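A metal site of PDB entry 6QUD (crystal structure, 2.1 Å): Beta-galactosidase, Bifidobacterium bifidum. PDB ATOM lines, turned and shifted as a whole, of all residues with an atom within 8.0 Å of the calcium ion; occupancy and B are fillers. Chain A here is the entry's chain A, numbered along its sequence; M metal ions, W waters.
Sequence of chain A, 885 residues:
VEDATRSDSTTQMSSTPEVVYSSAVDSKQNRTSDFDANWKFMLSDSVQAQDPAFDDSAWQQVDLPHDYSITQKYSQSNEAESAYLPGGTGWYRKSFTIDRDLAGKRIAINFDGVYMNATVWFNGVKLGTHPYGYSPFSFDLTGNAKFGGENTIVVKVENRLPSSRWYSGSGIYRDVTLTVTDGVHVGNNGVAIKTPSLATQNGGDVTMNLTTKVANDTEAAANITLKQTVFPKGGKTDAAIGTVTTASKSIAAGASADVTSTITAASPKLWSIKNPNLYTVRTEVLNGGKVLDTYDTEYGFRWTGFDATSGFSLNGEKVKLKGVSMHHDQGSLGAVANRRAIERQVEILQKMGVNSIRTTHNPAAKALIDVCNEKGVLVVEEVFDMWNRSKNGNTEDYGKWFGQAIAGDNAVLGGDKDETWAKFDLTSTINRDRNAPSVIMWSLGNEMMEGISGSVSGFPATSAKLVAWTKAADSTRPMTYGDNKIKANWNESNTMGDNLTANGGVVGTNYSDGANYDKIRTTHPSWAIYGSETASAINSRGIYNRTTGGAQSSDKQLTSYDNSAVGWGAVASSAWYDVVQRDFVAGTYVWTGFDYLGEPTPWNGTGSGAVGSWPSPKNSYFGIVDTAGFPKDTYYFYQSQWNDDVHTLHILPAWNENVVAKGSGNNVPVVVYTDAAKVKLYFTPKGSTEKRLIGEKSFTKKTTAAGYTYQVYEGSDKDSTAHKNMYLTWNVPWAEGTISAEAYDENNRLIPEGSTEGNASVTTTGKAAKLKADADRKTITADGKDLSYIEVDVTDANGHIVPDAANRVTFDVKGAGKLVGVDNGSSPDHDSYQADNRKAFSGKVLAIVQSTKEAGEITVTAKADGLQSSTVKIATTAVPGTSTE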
ATOM      1  N   TYR A 638      13.965 -15.207 -18.939  1.00  0.00           N
ATOM      2  CA  TYR A 638      14.375 -13.808 -19.051  1.00  0.00           C
ATOM      3  C   TYR A 638      13.179 -12.881 -19.127  1.00  0.00           C
ATOM      4  O   TYR A 638      13.158 -11.811 -18.506  1.00  0.00           O
ATOM      5  CB  TYR A 638      15.278 -13.626 -20.266  1.00  0.00           C
ATOM      6  CG  TYR A 638      16.698 -14.095 -20.053  1.00  0.00           C
ATOM      7  CD1 TYR A 638      17.569 -13.384 -19.233  1.00  0.00           C
ATOM      8  CD2 TYR A 638      17.171 -15.248 -20.669  1.00  0.00           C
ATOM      9  CE1 TYR A 638      18.866 -13.811 -19.036  1.00  0.00           C
ATOM     10  CE2 TYR A 638      18.478 -15.684 -20.468  1.00  0.00           C
ATOM     11  CZ  TYR A 638      19.317 -14.956 -19.656  1.00  0.00           C
ATOM     12  OH  TYR A 638      20.605 -15.365 -19.448  1.00  0.00           O
ATOM     13  N   GLN A 639      12.151 -13.274 -19.887  1.00  0.00           N
ATOM     14  CA  GLN A 639      10.967 -12.431 -20.015  1.00  0.00           C
ATOM     15  C   GLN A 639      10.262 -12.255 -18.671  1.00  0.00           C
ATOM     16  O   GLN A 639       9.752 -11.176 -18.365  1.00  0.00           O
ATOM     17  CB  GLN A 639      10.004 -13.031 -21.049  1.00  0.00           C
ATOM     18  CG  GLN A 639       8.854 -12.111 -21.428  1.00  0.00           C
ATOM     19  CD  GLN A 639       7.816 -12.810 -22.265  1.00  0.00           C
ATOM     20  OE1 GLN A 639       7.124 -13.709 -21.779  1.00  0.00           O
ATOM     21  NE2 GLN A 639       7.699 -12.415 -23.526  1.00  0.00           N
ATOM     22  N   SER A 640      10.220 -13.322 -17.861  1.00  0.00           N
ATOM     23  CA  SER A 640       9.669 -13.208 -16.518  1.00  0.00           C
ATOM     24  C   SER A 640      10.495 -12.295 -15.629  1.00  0.00           C
ATOM     25  O   SER A 640       9.972 -11.749 -14.653  1.00  0.00           O
ATOM     26  CB  SER A 640       9.566 -14.596 -15.867  1.00  0.00           C
ATOM     27  OG  SER A 640      10.851 -15.080 -15.527  1.00  0.00           O
ATOM     28  N   GLN A 641      11.781 -12.130 -15.945  1.00  0.00           N
ATOM     29  CA  GLN A 641      12.670 -11.277 -15.160  1.00  0.00           C
ATOM     30  C   GLN A 641      12.722  -9.847 -15.661  1.00  0.00           C
ATOM     31  O   GLN A 641      12.890  -8.927 -14.864  1.00  0.00           O
ATOM     32  CB  GLN A 641      14.086 -11.862 -15.169  1.00  0.00           C
ATOM     33  CG  GLN A 641      14.183 -13.279 -14.669  1.00  0.00           C
ATOM     34  CD  GLN A 641      13.619 -13.428 -13.282  1.00  0.00           C
ATOM     35  OE1 GLN A 641      14.126 -12.828 -12.337  1.00  0.00           O
ATOM     36  NE2 GLN A 641      12.564 -14.212 -13.146  1.00  0.00           N
ATOM     37  N   TRP A 642      12.583  -9.635 -16.970  1.00  0.00           N
ATOM     38  CA  TRP A 642      12.944  -8.372 -17.591  1.00  0.00           C
ATOM     39  C   TRP A 642      11.771  -7.573 -18.146  1.00  0.00           C
ATOM     40  O   TRP A 642      11.800  -6.344 -18.095  1.00  0.00           O
ATOM     41  CB  TRP A 642      13.941  -8.615 -18.733  1.00  0.00           C
ATOM     42  CG  TRP A 642      15.297  -9.018 -18.249  1.00  0.00           C
ATOM     43  CD1 TRP A 642      15.705  -9.121 -16.948  1.00  0.00           C
ATOM     44  CD2 TRP A 642      16.426  -9.369 -19.052  1.00  0.00           C
ATOM     45  NE1 TRP A 642      17.021  -9.520 -16.901  1.00  0.00           N
ATOM     46  CE2 TRP A 642      17.489  -9.678 -18.177  1.00  0.00           C
ATOM     47  CE3 TRP A 642      16.647  -9.447 -20.433  1.00  0.00           C
ATOM     48  CZ2 TRP A 642      18.744 -10.050 -18.634  1.00  0.00           C
ATOM     49  CZ3 TRP A 642      17.903  -9.824 -20.881  1.00  0.00           C
ATOM     50  CH2 TRP A 642      18.936 -10.119 -19.982  1.00  0.00           C
ATOM     51  N   ASN A 643      10.738  -8.227 -18.674  1.00  0.00           N
ATOM     52  CA  ASN A 643       9.680  -7.512 -19.378  1.00  0.00           C
ATOM     53  C   ASN A 643       8.569  -7.181 -18.390  1.00  0.00           C
ATOM     54  O   ASN A 643       7.780  -8.045 -18.010  1.00  0.00           O
ATOM     55  CB  ASN A 643       9.151  -8.336 -20.548  1.00  0.00           C
ATOM     56  CG  ASN A 643       8.327  -7.500 -21.517  1.00  0.00           C
ATOM     57  OD1 ASN A 643       7.785  -6.469 -21.141  1.00  0.00           O
ATOM     58  ND2 ASN A 643       8.257  -7.952 -22.764  1.00  0.00           N
ATOM     59  N   ASP A 644       8.507  -5.920 -17.979  1.00  0.00           N
ATOM     60  CA  ASP A 644       7.479  -5.457 -17.064  1.00  0.00           C
ATOM     61  C   ASP A 644       6.215  -4.971 -17.770  1.00  0.00           C
ATOM     62  O   ASP A 644       5.307  -4.475 -17.111  1.00  0.00           O
ATOM     63  CB  ASP A 644       8.035  -4.342 -16.169  1.00  0.00           C
ATOM     64  CG  ASP A 644       9.226  -4.792 -15.349  1.00  0.00           C
ATOM     65  OD1 ASP A 644       9.267  -5.978 -14.938  1.00  0.00           O
ATOM     66  OD2 ASP A 644      10.139  -3.961 -15.121  1.00  0.00           O
ATOM     67  N   ASP A 645       6.146  -5.106 -19.097  1.00  0.00           N
ATOM     68  CA  ASP A 645       4.958  -4.752 -19.869  1.00  0.00           C
ATOM     69  C   ASP A 645       4.087  -5.947 -20.204  1.00  0.00           C
ATOM     70  O   ASP A 645       2.973  -5.757 -20.709  1.00  0.00           O
ATOM     71  CB  ASP A 645       5.362  -4.043 -21.168  1.00  0.00           C
ATOM     72  CG  ASP A 645       5.810  -2.615 -20.940  1.00  0.00           C
ATOM     73  OD1 ASP A 645       5.645  -2.116 -19.808  1.00  0.00           O
ATOM     74  OD2 ASP A 645       6.336  -1.998 -21.888  1.00  0.00           O
ATOM     75  N   VAL A 646       4.551  -7.172 -19.946  1.00  0.00           N
ATOM     76  CA  VAL A 646       3.785  -8.380 -20.210  1.00  0.00           C
ATOM     77  C   VAL A 646       3.870  -9.281 -18.977  1.00  0.00           C
ATOM     78  O   VAL A 646       4.700  -9.088 -18.086  1.00  0.00           O
ATOM     79  CB  VAL A 646       4.281  -9.137 -21.460  1.00  0.00           C
ATOM     80  CG1 VAL A 646       4.387  -8.207 -22.656  1.00  0.00           C
ATOM     81  CG2 VAL A 646       5.610  -9.816 -21.173  1.00  0.00           C
ATOM     82  N   HIS A 647       2.996 -10.282 -18.949  1.00  0.00           N
ATOM     83  CA  HIS A 647       3.038 -11.322 -17.934  1.00  0.00           C
ATOM     84  C   HIS A 647       3.476 -12.624 -18.587  1.00  0.00           C
ATOM     85  O   HIS A 647       3.111 -12.914 -19.731  1.00  0.00           O
ATOM     86  CB  HIS A 647       1.674 -11.494 -17.259  1.00  0.00           C
ATOM     87  CG  HIS A 647       1.246 -10.311 -16.467  1.00  0.00           C
ATOM     88  ND1 HIS A 647       2.140  -9.512 -15.785  1.00  0.00           N
ATOM     89  CD2 HIS A 647       0.019  -9.768 -16.240  1.00  0.00           C
ATOM     90  CE1 HIS A 647       1.489  -8.541 -15.172  1.00  0.00           C
ATOM     91  NE2 HIS A 647       0.201  -8.669 -15.431  1.00  0.00           N
ATOM     92  N   THR A 648       4.281 -13.409 -17.867  1.00  0.00           N
ATOM     93  CA  THR A 648       4.862 -14.626 -18.395  1.00  0.00           C
ATOM     94  C   THR A 648       4.368 -15.822 -17.587  1.00  0.00           C
ATOM     95  O   THR A 648       4.273 -15.763 -16.364  1.00  0.00           O
ATOM     96  CB  THR A 648       6.396 -14.565 -18.351  1.00  0.00           C
ATOM     97  OG1 THR A 648       6.838 -13.374 -19.026  1.00  0.00           O
ATOM     98  CG2 THR A 648       7.012 -15.780 -19.036  1.00  0.00           C
ATOM     99  N   THR A 674       7.790 -17.619 -14.681  1.00  0.00           N
ATOM    100  CA  THR A 674       6.653 -16.731 -14.519  1.00  0.00           C
ATOM    101  C   THR A 674       7.061 -15.518 -13.708  1.00  0.00           C
ATOM    102  O   THR A 674       8.032 -15.562 -12.931  1.00  0.00           O
ATOM    103  CB  THR A 674       5.473 -17.454 -13.846  1.00  0.00           C
ATOM    104  OG1 THR A 674       4.335 -16.586 -13.813  1.00  0.00           O
ATOM    105  CG2 THR A 674       5.837 -17.861 -12.415  1.00  0.00           C
ATOM    106  N   ASP A 675       6.321 -14.428 -13.891  1.00  0.00           N
ATOM    107  CA  ASP A 675       6.481 -13.232 -13.068  1.00  0.00           C
ATOM    108  C   ASP A 675       5.347 -13.068 -12.072  1.00  0.00           C
ATOM    109  O   ASP A 675       5.355 -12.095 -11.302  1.00  0.00           O
ATOM    110  CB  ASP A 675       6.582 -11.983 -13.955  1.00  0.00           C
ATOM    111  CG  ASP A 675       5.334 -11.755 -14.794  1.00  0.00           C
ATOM    112  OD1 ASP A 675       4.694 -12.757 -15.187  1.00  0.00           O
ATOM    113  OD2 ASP A 675       5.001 -10.585 -15.056  1.00  0.00           O
ATOM    114  N   ALA A 676       4.389 -13.989 -12.031  1.00  0.00           N
ATOM    115  CA  ALA A 676       3.289 -13.911 -11.091  1.00  0.00           C
ATOM    116  C   ALA A 676       3.775 -14.152  -9.671  1.00  0.00           C
ATOM    117  O   ALA A 676       4.846 -14.713  -9.429  1.00  0.00           O
ATOM    118  CB  ALA A 676       2.201 -14.927 -11.440  1.00  0.00           C
HETATM  119 CA    CA M   1       6.341  -9.048 -16.401  1.00  0.00          CA
HETATM  120  O   HOH W   1       6.960 -11.165 -17.521  1.00  0.00           O
HETATM  121  O   HOH W   2       8.494  -9.092 -15.168  1.00  0.00           O
HETATM  122  O   HOH W   3       5.246  -7.240 -15.036  1.00  0.00           O
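Residues that only touch the calcium ion: Asp 644.
O of Val 646 is bound to the calcium ion, at 2.4 Å.
The calcium ion is bound by the backbone carbonyl oxygen (O) of Asn 643, 2.4 Å away.
The calcium ion is bound by OD2 of Asp 675 (2.4 Å).
The calcium ion is bound by water W1 (2.5 Å).
The calcium ion is bound by water W2, 2.5 Å away.
Water W3 binds the calcium ion (2.5 Å).
Water W2 bridges the backbone carbonyl oxygen (O) of Ser 640 and the side-chain carboxylate (OD1) of Asp 644.
Water W1 bridges OG1 of Thr 648 (2.7 Å) and O of Gln 639 (2.9 Å).
The backbone NH (N) of Thr 648 is in hydrogen-bond range of the side-chain carboxylate (OD1) of Asp 675, 2.8 Å away.
OD1 of Asn 643 is in hydrogen-bond range of N of Asp 645 (3.0 Å).
ND1 of His 647 lies close to OD2 of Asp 675, 3.1 Å away.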
